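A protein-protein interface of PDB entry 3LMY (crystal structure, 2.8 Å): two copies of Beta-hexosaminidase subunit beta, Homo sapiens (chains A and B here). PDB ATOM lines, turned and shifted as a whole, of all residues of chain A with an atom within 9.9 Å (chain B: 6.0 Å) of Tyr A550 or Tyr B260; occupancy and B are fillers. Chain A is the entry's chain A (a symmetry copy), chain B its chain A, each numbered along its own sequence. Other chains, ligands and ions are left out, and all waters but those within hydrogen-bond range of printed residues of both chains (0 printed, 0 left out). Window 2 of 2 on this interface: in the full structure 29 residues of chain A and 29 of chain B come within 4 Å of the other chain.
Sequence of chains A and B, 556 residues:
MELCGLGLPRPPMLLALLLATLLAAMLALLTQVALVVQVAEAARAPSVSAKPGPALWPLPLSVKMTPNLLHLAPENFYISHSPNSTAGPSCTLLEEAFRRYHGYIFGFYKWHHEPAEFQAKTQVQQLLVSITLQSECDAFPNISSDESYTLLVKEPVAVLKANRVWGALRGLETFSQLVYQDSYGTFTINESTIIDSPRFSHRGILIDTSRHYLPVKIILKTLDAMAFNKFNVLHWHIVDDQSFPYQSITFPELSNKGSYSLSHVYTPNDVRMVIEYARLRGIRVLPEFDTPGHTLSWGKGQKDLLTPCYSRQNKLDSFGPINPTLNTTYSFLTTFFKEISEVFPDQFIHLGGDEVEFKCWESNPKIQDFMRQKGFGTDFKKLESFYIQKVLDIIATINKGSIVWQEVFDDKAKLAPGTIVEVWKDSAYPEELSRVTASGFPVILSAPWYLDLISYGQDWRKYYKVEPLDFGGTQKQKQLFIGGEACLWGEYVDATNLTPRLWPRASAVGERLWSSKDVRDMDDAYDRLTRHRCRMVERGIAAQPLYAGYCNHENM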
ATOM      1  N   TYR A 526      20.212  10.214  22.249  1.00  0.00           N
ATOM      2  CA  TYR A 526      19.255   9.122  22.185  1.00  0.00           C
ATOM      3  C   TYR A 526      17.899   9.652  21.898  1.00  0.00           C
ATOM      4  O   TYR A 526      17.124   9.111  21.106  1.00  0.00           O
ATOM      5  CB  TYR A 526      19.168   8.376  23.490  1.00  0.00           C
ATOM      6  CG  TYR A 526      18.200   7.246  23.353  1.00  0.00           C
ATOM      7  CD1 TYR A 526      18.440   6.205  22.446  1.00  0.00           C
ATOM      8  CD2 TYR A 526      16.997   7.234  24.079  1.00  0.00           C
ATOM      9  CE1 TYR A 526      17.514   5.173  22.297  1.00  0.00           C
ATOM     10  CE2 TYR A 526      16.081   6.221  23.933  1.00  0.00           C
ATOM     11  CZ  TYR A 526      16.345   5.199  23.046  1.00  0.00           C
ATOM     12  OH  TYR A 526      15.445   4.191  22.917  1.00  0.00           O
ATOM     13  N   THR A 530      15.917   9.153  18.236  1.00  0.00           N
ATOM     14  CA  THR A 530      14.746   8.280  18.104  1.00  0.00           C
ATOM     15  C   THR A 530      13.682   9.072  17.369  1.00  0.00           C
ATOM     16  O   THR A 530      13.031   8.546  16.463  1.00  0.00           O
ATOM     17  CB  THR A 530      14.174   7.818  19.453  1.00  0.00           C
ATOM     18  OG1 THR A 530      14.189   8.937  20.311  1.00  0.00           O
ATOM     19  CG2 THR A 530      15.025   6.750  20.121  1.00  0.00           C
ATOM     20  N   ARG A 531      13.540  10.349  17.739  1.00  0.00           N
ATOM     21  CA  ARG A 531      12.568  11.259  17.125  1.00  0.00           C
ATOM     22  C   ARG A 531      12.906  11.628  15.663  1.00  0.00           C
ATOM     23  O   ARG A 531      12.033  11.588  14.792  1.00  0.00           O
ATOM     24  CB  ARG A 531      12.310  12.443  18.043  1.00  0.00           C
ATOM     25  CG  ARG A 531      11.468  11.935  19.239  1.00  0.00           C
ATOM     26  CD  ARG A 531      11.631  12.659  20.571  1.00  0.00           C
ATOM     27  NE  ARG A 531      11.155  14.031  20.422  1.00  0.00           N
ATOM     28  CZ  ARG A 531      11.887  15.133  20.615  1.00  0.00           C
ATOM     29  NH1 ARG A 531      13.162  15.068  21.037  1.00  0.00           N
ATOM     30  NH2 ARG A 531      11.321  16.323  20.396  1.00  0.00           N
ATOM     31  N   ARG A 533      14.583   9.680  13.669  1.00  0.00           N
ATOM     32  CA  ARG A 533      14.336   8.452  12.951  1.00  0.00           C
ATOM     33  C   ARG A 533      12.866   8.316  12.574  1.00  0.00           C
ATOM     34  O   ARG A 533      12.591   7.971  11.431  1.00  0.00           O
ATOM     35  CB  ARG A 533      14.852   7.253  13.748  1.00  0.00           C
ATOM     36  CG  ARG A 533      14.614   5.912  13.112  1.00  0.00           C
ATOM     37  CD  ARG A 533      13.470   5.191  13.784  1.00  0.00           C
ATOM     38  NE  ARG A 533      13.054   4.088  12.937  1.00  0.00           N
ATOM     39  CZ  ARG A 533      12.142   3.187  13.280  1.00  0.00           C
ATOM     40  NH1 ARG A 533      11.579   3.276  14.453  1.00  0.00           N
ATOM     41  NH2 ARG A 533      11.816   2.185  12.459  1.00  0.00           N
ATOM     42  N   CYS A 534      11.937   8.608  13.489  1.00  0.00           N
ATOM     43  CA  CYS A 534      10.528   8.590  13.121  1.00  0.00           C
ATOM     44  C   CYS A 534      10.185   9.539  11.983  1.00  0.00           C
ATOM     45  O   CYS A 534       9.302   9.234  11.137  1.00  0.00           O
ATOM     46  CB  CYS A 534       9.642   8.967  14.278  1.00  0.00           C
ATOM     47  SG  CYS A 534       9.460   7.670  15.498  1.00  0.00           S
ATOM     48  N   ARG A 535      10.859  10.693  11.987  1.00  0.00           N
ATOM     49  CA  ARG A 535      10.720  11.697  10.944  1.00  0.00           C
ATOM     50  C   ARG A 535      11.117  11.106   9.620  1.00  0.00           C
ATOM     51  O   ARG A 535      10.373  11.203   8.672  1.00  0.00           O
ATOM     52  CB  ARG A 535      11.597  12.907  11.263  1.00  0.00           C
ATOM     53  CG  ARG A 535      11.462  14.039  10.264  1.00  0.00           C
ATOM     54  CD  ARG A 535      11.724  15.386  10.889  1.00  0.00           C
ATOM     55  NE  ARG A 535      13.001  15.296  11.565  1.00  0.00           N
ATOM     56  CZ  ARG A 535      13.351  16.013  12.618  1.00  0.00           C
ATOM     57  NH1 ARG A 535      12.522  16.919  13.135  1.00  0.00           N
ATOM     58  NH2 ARG A 535      14.540  15.797  13.141  1.00  0.00           N
ATOM     59  N   VAL A 537      11.251   7.940   8.731  1.00  0.00           N
ATOM     60  CA  VAL A 537      10.235   6.951   8.394  1.00  0.00           C
ATOM     61  C   VAL A 537       9.018   7.657   7.794  1.00  0.00           C
ATOM     62  O   VAL A 537       8.442   7.209   6.799  1.00  0.00           O
ATOM     63  CB  VAL A 537       9.849   6.115   9.630  1.00  0.00           C
ATOM     64  CG1 VAL A 537       8.727   5.256   9.338  1.00  0.00           C
ATOM     65  CG2 VAL A 537      11.015   5.264  10.073  1.00  0.00           C
ATOM     66  N   PRO A 545      14.826   0.672  13.791  1.00  0.00           N
ATOM     67  CA  PRO A 545      14.729   1.247  15.136  1.00  0.00           C
ATOM     68  C   PRO A 545      16.094   1.430  15.855  1.00  0.00           C
ATOM     69  O   PRO A 545      17.109   0.883  15.412  1.00  0.00           O
ATOM     70  CB  PRO A 545      13.897   0.214  15.891  1.00  0.00           C
ATOM     71  CG  PRO A 545      13.231  -0.556  14.893  1.00  0.00           C
ATOM     72  CD  PRO A 545      14.091  -0.592  13.684  1.00  0.00           C
ATOM     73  N   LEU A 546      16.113   2.205  16.947  1.00  0.00           N
ATOM     74  CA  LEU A 546      17.283   2.321  17.833  1.00  0.00           C
ATOM     75  C   LEU A 546      17.143   1.313  18.984  1.00  0.00           C
ATOM     76  O   LEU A 546      18.140   0.712  19.448  1.00  0.00           O
ATOM     77  CB  LEU A 546      17.383   3.741  18.413  1.00  0.00           C
ATOM     78  CG  LEU A 546      17.905   4.915  17.592  1.00  0.00           C
ATOM     79  CD1 LEU A 546      18.067   6.143  18.439  1.00  0.00           C
ATOM     80  CD2 LEU A 546      19.259   4.566  17.063  1.00  0.00           C
ATOM     81  N   TYR A 547      15.894   1.159  19.439  1.00  0.00           N
ATOM     82  CA  TYR A 547      15.560   0.302  20.545  1.00  0.00           C
ATOM     83  C   TYR A 547      14.015   0.125  20.602  1.00  0.00           C
ATOM     84  O   TYR A 547      13.321   0.565  19.685  1.00  0.00           O
ATOM     85  CB  TYR A 547      16.207   0.822  21.842  1.00  0.00           C
ATOM     86  CG  TYR A 547      16.040  -0.107  23.033  1.00  0.00           C
ATOM     87  CD1 TYR A 547      16.490  -1.431  22.986  1.00  0.00           C
ATOM     88  CD2 TYR A 547      15.410   0.334  24.194  1.00  0.00           C
ATOM     89  CE1 TYR A 547      16.320  -2.288  24.046  1.00  0.00           C
ATOM     90  CE2 TYR A 547      15.232  -0.505  25.271  1.00  0.00           C
ATOM     91  CZ  TYR A 547      15.697  -1.828  25.204  1.00  0.00           C
ATOM     92  OH  TYR A 547      15.523  -2.672  26.307  1.00  0.00           O
ATOM     93  N   ALA A 548      13.486  -0.569  21.617  1.00  0.00           N
ATOM     94  CA  ALA A 548      12.055  -0.804  21.756  1.00  0.00           C
ATOM     95  C   ALA A 548      11.294   0.517  21.685  1.00  0.00           C
ATOM     96  O   ALA A 548      11.846   1.532  22.010  1.00  0.00           O
ATOM     97  CB  ALA A 548      11.777  -1.506  23.070  1.00  0.00           C
ATOM     98  N   GLY A 549      10.037   0.494  21.234  1.00  0.00           N
ATOM     99  CA  GLY A 549       9.172   1.696  21.166  1.00  0.00           C
ATOM    100  C   GLY A 549       8.214   1.734  20.003  1.00  0.00           C
ATOM    101  O   GLY A 549       7.925   0.697  19.408  1.00  0.00           O
ATOM    102  N   TYR A 550       7.741   2.931  19.652  1.00  0.00           N
ATOM    103  CA  TYR A 550       6.844   3.126  18.476  1.00  0.00           C
ATOM    104  C   TYR A 550       6.841   4.550  17.925  1.00  0.00           C
ATOM    105  O   TYR A 550       7.339   5.434  18.594  1.00  0.00           O
ATOM    106  CB  TYR A 550       5.427   2.800  18.892  1.00  0.00           C
ATOM    107  CG  TYR A 550       4.802   3.823  19.812  1.00  0.00           C
ATOM    108  CD1 TYR A 550       5.276   4.029  21.112  1.00  0.00           C
ATOM    109  CD2 TYR A 550       3.710   4.572  19.382  1.00  0.00           C
ATOM    110  CE1 TYR A 550       4.669   4.947  21.944  1.00  0.00           C
ATOM    111  CE2 TYR A 550       3.087   5.486  20.214  1.00  0.00           C
ATOM    112  CZ  TYR A 550       3.564   5.667  21.483  1.00  0.00           C
ATOM    113  OH  TYR A 550       2.919   6.589  22.262  1.00  0.00           O
ATOM    114  N   CYS A 551       6.237   4.807  16.754  1.00  0.00           N
ATOM    115  CA  CYS A 551       6.005   6.236  16.386  1.00  0.00           C
ATOM    116  C   CYS A 551       4.596   6.847  16.559  1.00  0.00           C
ATOM    117  O   CYS A 551       3.592   6.117  16.565  1.00  0.00           O
ATOM    118  CB  CYS A 551       6.486   6.539  14.995  1.00  0.00           C
ATOM    119  SG  CYS A 551       8.171   6.114  14.787  1.00  0.00           S
ATOM    120  N   ASN A 552       4.572   8.199  16.680  1.00  0.00           N
ATOM    121  CA  ASN A 552       3.369   9.130  16.646  1.00  0.00           C
ATOM    122  C   ASN A 552       3.065   9.805  17.998  1.00  0.00           C
ATOM    123  O   ASN A 552       3.891   9.793  18.926  1.00  0.00           O
ATOM    124  CB  ASN A 552       2.075   8.539  15.968  1.00  0.00           C
ATOM    125  CG  ASN A 552       2.206   8.377  14.395  1.00  0.00           C
ATOM    126  OD1 ASN A 552       2.744   9.252  13.707  1.00  0.00           O
ATOM    127  ND2 ASN A 552       1.707   7.259  13.854  1.00  0.00           N
ATOM    128  N   THR B 209       6.112  -9.171  19.214  1.00  0.00           N
ATOM    129  CA  THR B 209       5.253  -8.051  18.835  1.00  0.00           C
ATOM    130  C   THR B 209       5.029  -7.126  20.002  1.00  0.00           C
ATOM    131  O   THR B 209       4.040  -6.429  20.027  1.00  0.00           O
ATOM    132  CB  THR B 209       3.878  -8.496  18.364  1.00  0.00           C
ATOM    133  OG1 THR B 209       3.346  -9.429  19.313  1.00  0.00           O
ATOM    134  CG2 THR B 209       3.929  -9.140  16.957  1.00  0.00           C
ATOM    135  N   SER B 210       5.926  -7.155  20.989  1.00  0.00           N
ATOM    136  CA  SER B 210       5.852  -6.273  22.130  1.00  0.00           C
ATOM    137  C   SER B 210       6.969  -5.216  22.090  1.00  0.00           C
ATOM    138  O   SER B 210       6.690  -4.011  22.120  1.00  0.00           O
ATOM    139  CB  SER B 210       5.911  -7.060  23.428  1.00  0.00           C
ATOM    140  OG  SER B 210       5.903  -6.178  24.558  1.00  0.00           O
ATOM    141  N   ARG B 211       8.229  -5.645  22.029  1.00  0.00           N
ATOM    142  CA  ARG B 211       9.322  -4.686  21.864  1.00  0.00           C
ATOM    143  C   ARG B 211       9.017  -3.671  20.724  1.00  0.00           C
ATOM    144  O   ARG B 211       9.248  -2.461  20.872  1.00  0.00           O
ATOM    145  CB  ARG B 211      10.645  -5.413  21.667  1.00  0.00           C
ATOM    146  CG  ARG B 211      11.318  -5.816  22.967  1.00  0.00           C
ATOM    147  CD  ARG B 211      10.375  -6.598  23.857  1.00  0.00           C
ATOM    148  NE  ARG B 211      11.037  -7.135  25.039  1.00  0.00           N
ATOM    149  CZ  ARG B 211      11.613  -8.338  25.123  1.00  0.00           C
ATOM    150  NH1 ARG B 211      11.611  -9.182  24.093  1.00  0.00           N
ATOM    151  NH2 ARG B 211      12.207  -8.703  26.250  1.00  0.00           N
ATOM    152  N   HIS B 212       8.460  -4.180  19.624  1.00  0.00           N
ATOM    153  CA  HIS B 212       7.818  -3.386  18.580  1.00  0.00           C
ATOM    154  C   HIS B 212       6.506  -4.010  18.146  1.00  0.00           C
ATOM    155  O   HIS B 212       6.356  -5.240  18.151  1.00  0.00           O
ATOM    156  CB  HIS B 212       8.759  -3.270  17.387  1.00  0.00           C
ATOM    157  CG  HIS B 212       9.888  -2.339  17.642  1.00  0.00           C
ATOM    158  ND1 HIS B 212      11.149  -2.777  17.965  1.00  0.00           N
ATOM    159  CD2 HIS B 212       9.923  -0.992  17.731  1.00  0.00           C
ATOM    160  CE1 HIS B 212      11.929  -1.735  18.189  1.00  0.00           C
ATOM    161  NE2 HIS B 212      11.207  -0.640  18.055  1.00  0.00           N
ATOM    162  N   TYR B 213       5.540  -3.190  17.766  1.00  0.00           N
ATOM    163  CA  TYR B 213       4.275  -3.760  17.298  1.00  0.00           C
ATOM    164  C   TYR B 213       4.388  -4.084  15.808  1.00  0.00           C
ATOM    165  O   TYR B 213       4.712  -3.233  15.011  1.00  0.00           O
ATOM    166  CB  TYR B 213       3.126  -2.789  17.561  1.00  0.00           C
ATOM    167  CG  TYR B 213       1.779  -3.133  16.909  1.00  0.00           C
ATOM    168  CD1 TYR B 213       0.840  -3.920  17.590  1.00  0.00           C
ATOM    169  CD2 TYR B 213       1.425  -2.631  15.641  1.00  0.00           C
ATOM    170  CE1 TYR B 213      -0.383  -4.209  17.024  1.00  0.00           C
ATOM    171  CE2 TYR B 213       0.216  -2.922  15.071  1.00  0.00           C
ATOM    172  CZ  TYR B 213      -0.684  -3.699  15.777  1.00  0.00           C
ATOM    173  OH  TYR B 213      -1.902  -4.037  15.252  1.00  0.00           O
ATOM    174  N   GLN B 242       7.494  -4.102  27.595  1.00  0.00           N
ATOM    175  CA  GLN B 242       7.315  -2.812  26.947  1.00  0.00           C
ATOM    176  C   GLN B 242       5.932  -2.469  26.488  1.00  0.00           C
ATOM    177  O   GLN B 242       5.605  -1.301  26.417  1.00  0.00           O
ATOM    178  CB  GLN B 242       8.233  -2.671  25.751  1.00  0.00           C
ATOM    179  CG  GLN B 242       9.672  -2.482  26.123  1.00  0.00           C
ATOM    180  CD  GLN B 242      10.389  -3.799  26.388  1.00  0.00           C
ATOM    181  OE1 GLN B 242       9.796  -4.787  26.805  1.00  0.00           O
ATOM    182  NE2 GLN B 242      11.682  -3.803  26.161  1.00  0.00           N
ATOM    183  N   SER B 243       5.125  -3.443  26.106  1.00  0.00           N
ATOM    184  CA  SER B 243       3.799  -3.121  25.578  1.00  0.00           C
ATOM    185  C   SER B 243       2.943  -4.363  25.586  1.00  0.00           C
ATOM    186  O   SER B 243       3.470  -5.480  25.378  1.00  0.00           O
ATOM    187  CB  SER B 243       3.869  -2.501  24.163  1.00  0.00           C
ATOM    188  OG  SER B 243       4.193  -3.447  23.157  1.00  0.00           O
ATOM    189  N   PHE B 244       1.640  -4.174  25.825  1.00  0.00           N
ATOM    190  CA  PHE B 244       0.662  -5.275  25.831  1.00  0.00           C
ATOM    191  C   PHE B 244      -0.350  -5.103  24.684  1.00  0.00           C
ATOM    192  O   PHE B 244      -1.485  -4.704  24.937  1.00  0.00           O
ATOM    193  CB  PHE B 244      -0.070  -5.303  27.177  1.00  0.00           C
ATOM    194  CG  PHE B 244      -0.724  -6.629  27.511  1.00  0.00           C
ATOM    195  CD1 PHE B 244      -1.919  -7.014  26.911  1.00  0.00           C
ATOM    196  CD2 PHE B 244      -0.164  -7.482  28.490  1.00  0.00           C
ATOM    197  CE1 PHE B 244      -2.531  -8.246  27.269  1.00  0.00           C
ATOM    198  CE2 PHE B 244      -0.766  -8.719  28.847  1.00  0.00           C
ATOM    199  CZ  PHE B 244      -1.945  -9.095  28.244  1.00  0.00           C
ATOM    200  N   PRO B 245       0.059  -5.408  23.420  1.00  0.00           N
ATOM    201  CA  PRO B 245      -0.821  -5.223  22.250  1.00  0.00           C
ATOM    202  C   PRO B 245      -2.018  -6.210  22.103  1.00  0.00           C
ATOM    203  O   PRO B 245      -2.910  -5.923  21.283  1.00  0.00           O
ATOM    204  CB  PRO B 245       0.135  -5.367  21.075  1.00  0.00           C
ATOM    205  CG  PRO B 245       1.218  -6.249  21.560  1.00  0.00           C
ATOM    206  CD  PRO B 245       1.300  -6.119  23.047  1.00  0.00           C
ATOM    207  N   SER B 255      -4.952  -4.313  27.643  1.00  0.00           N
ATOM    208  CA  SER B 255      -4.461  -3.663  26.454  1.00  0.00           C
ATOM    209  C   SER B 255      -4.744  -2.130  26.421  1.00  0.00           C
ATOM    210  O   SER B 255      -3.902  -1.330  25.940  1.00  0.00           O
ATOM    211  CB  SER B 255      -4.907  -4.389  25.199  1.00  0.00           C
ATOM    212  OG  SER B 255      -6.159  -3.931  24.812  1.00  0.00           O
ATOM    213  N   GLY B 258      -1.931  -0.913  28.504  1.00  0.00           N
ATOM    214  CA  GLY B 258      -0.601  -1.476  28.312  1.00  0.00           C
ATOM    215  C   GLY B 258      -0.114  -1.457  26.870  1.00  0.00           C
ATOM    216  O   GLY B 258       1.088  -1.591  26.594  1.00  0.00           O
ATOM    217  N   SER B 259      -1.035  -1.303  25.933  1.00  0.00           N
ATOM    218  CA  SER B 259      -0.629  -1.218  24.563  1.00  0.00           C
ATOM    219  C   SER B 259       0.114   0.102  24.300  1.00  0.00           C
ATOM    220  O   SER B 259      -0.025   1.027  25.068  1.00  0.00           O
ATOM    221  CB  SER B 259      -1.848  -1.309  23.709  1.00  0.00           C
ATOM    222  OG  SER B 259      -2.347  -0.012  23.513  1.00  0.00           O
ATOM    223  N   TYR B 260       0.902   0.200  23.226  1.00  0.00           N
ATOM    224  CA  TYR B 260       1.624   1.447  22.940  1.00  0.00           C
ATOM    225  C   TYR B 260       0.677   2.620  22.671  1.00  0.00           C
ATOM    226  O   TYR B 260       0.979   3.759  23.012  1.00  0.00           O
ATOM    227  CB  TYR B 260       2.558   1.281  21.768  1.00  0.00           C
ATOM    228  CG  TYR B 260       3.900   0.632  22.063  1.00  0.00           C
ATOM    229  CD1 TYR B 260       4.737   1.134  23.061  1.00  0.00           C
ATOM    230  CD2 TYR B 260       4.378  -0.443  21.278  1.00  0.00           C
ATOM    231  CE1 TYR B 260       5.986   0.579  23.306  1.00  0.00           C
ATOM    232  CE2 TYR B 260       5.631  -1.004  21.526  1.00  0.00           C
ATOM    233  CZ  TYR B 260       6.417  -0.481  22.549  1.00  0.00           C
ATOM    234  OH  TYR B 260       7.656  -1.022  22.823  1.00  0.00           O
ATOM    235  N   SER B 261      -0.476   2.325  22.077  1.00  0.00           N
ATOM    236  CA  SER B 261      -1.506   3.312  21.736  1.00  0.00           C
ATOM    237  C   SER B 261      -2.672   2.481  21.271  1.00  0.00           C
ATOM    238  O   SER B 261      -2.513   1.290  21.052  1.00  0.00           O
ATOM    239  CB  SER B 261      -1.072   4.283  20.606  1.00  0.00           C
ATOM    240  OG  SER B 261      -1.250   3.749  19.281  1.00  0.00           O
ATOM    241  N   LEU B 262      -3.834   3.107  21.101  1.00  0.00           N
ATOM    242  CA  LEU B 262      -5.034   2.388  20.681  1.00  0.00           C
ATOM    243  C   LEU B 262      -4.868   1.745  19.343  1.00  0.00           C
ATOM    244  O   LEU B 262      -5.503   0.729  19.086  1.00  0.00           O
ATOM    245  CB  LEU B 262      -6.270   3.282  20.694  1.00  0.00           C
ATOM    246  CG  LEU B 262      -7.078   3.346  22.022  1.00  0.00           C
ATOM    247  CD1 LEU B 262      -6.488   2.661  23.335  1.00  0.00           C
ATOM    248  CD2 LEU B 262      -7.401   4.830  22.265  1.00  0.00           C
ATOM    249  N   HIS B 264      -2.039   0.210  18.264  1.00  0.00           N
ATOM    250  CA  HIS B 264      -1.011  -0.838  18.315  1.00  0.00           C
ATOM    251  C   HIS B 264      -1.581  -1.949  19.135  1.00  0.00           C
ATOM    252  O   HIS B 264      -1.090  -2.280  20.215  1.00  0.00           O
ATOM    253  CB  HIS B 264       0.292  -0.348  18.920  1.00  0.00           C
ATOM    254  CG  HIS B 264       0.906   0.769  18.152  1.00  0.00           C
ATOM    255  ND1 HIS B 264       0.514   2.083  18.309  1.00  0.00           N
ATOM    256  CD2 HIS B 264       1.863   0.770  17.191  1.00  0.00           C
ATOM    257  CE1 HIS B 264       1.223   2.848  17.491  1.00  0.00           C
ATOM    258  NE2 HIS B 264       2.051   2.077  16.802  1.00  0.00           N
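The backbone carbonyl oxygen (O) of Tyr A547 lies within hydrogen-bond range of a ring nitrogen (NE2) of His B212 (2.9 Å).
N of Gly A549 sits at hydrogen-bond distance from O of Arg B211, 3.1 Å away.
The side-chain hydroxyl (OH) of Tyr B260 lies within hydrogen-bond range of the backbone NH (N) of Gly A549 (3.2 Å).
The side-chain amide oxygen of Gln B242 is in hydrogen-bond range of the guanidinium group of Arg B211 (3.2 Å).
The side-chain sulfur (SG) of Cys A551 is disulfide-bonded to the side-chain sulfur (SG) of Cys A534, 2.1 Å away.
The backbone carbonyl oxygen of Ser B210 is in hydrogen-bond range of the side-chain hydroxyl of Tyr B260.
O of Arg B211 is in hydrogen-bond range of OH of Tyr B260.
The side-chain hydroxyl of Ser B261 lies within hydrogen-bond range of a ring nitrogen (ND1) of His B264 (2.6 Å).
Among the printed residues, pairs that only touch across the chains: Pro A545 with His B212 (3.6 Å), Ala A548 with Arg B211 (3.4 Å), Ala A548 with His B212 (3.7 Å), Ala A548 with Gln B242 (3.8 Å), Gly A549 with His B212 (3.1 Å), Tyr A550 with Tyr B260 (3.5 Å) and Tyr A550 with His B264 (3.6 Å).
Of chain B, only Tyr B260 (3.5 Å) and His B264 (3.6 Å) come within 4 Å of Tyr A550.
Tyr B260 touches just these residues of chain A: Gly A549 (3.2 Å) and Tyr A550 (3.5 Å).
No residue of chain A comes within 4 Å of Ser B259.
Ser B261 touches none of the printed residues of chain A.
His B264 touches one residue of chain A.
Of the printed residues of chain A, His B212 touches Pro A545 (3.6 Å), Tyr A547 (2.9 Å), Ala A548 (3.7 Å) and Gly A549 (3.1 Å).
Printed residues of chain B within 4 Å of Gly A549: Arg B211, His B212 and Tyr B260.
Ser B255 touches none of the printed residues of chain A.
Hydrophobic or aromatic side chains of chain B that line the printed part of chain A: His B212, Tyr B260 and His B264.
Hydrophobic or aromatic side chains of chain A within 4 Å of the printed part of chain B: Pro A545, Ala A548 and Tyr A550.
No position is printed for both chains.
Of the 10 pairs that touch across the chains among the printed residues, none has its exchanged pair printed and touching as well.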
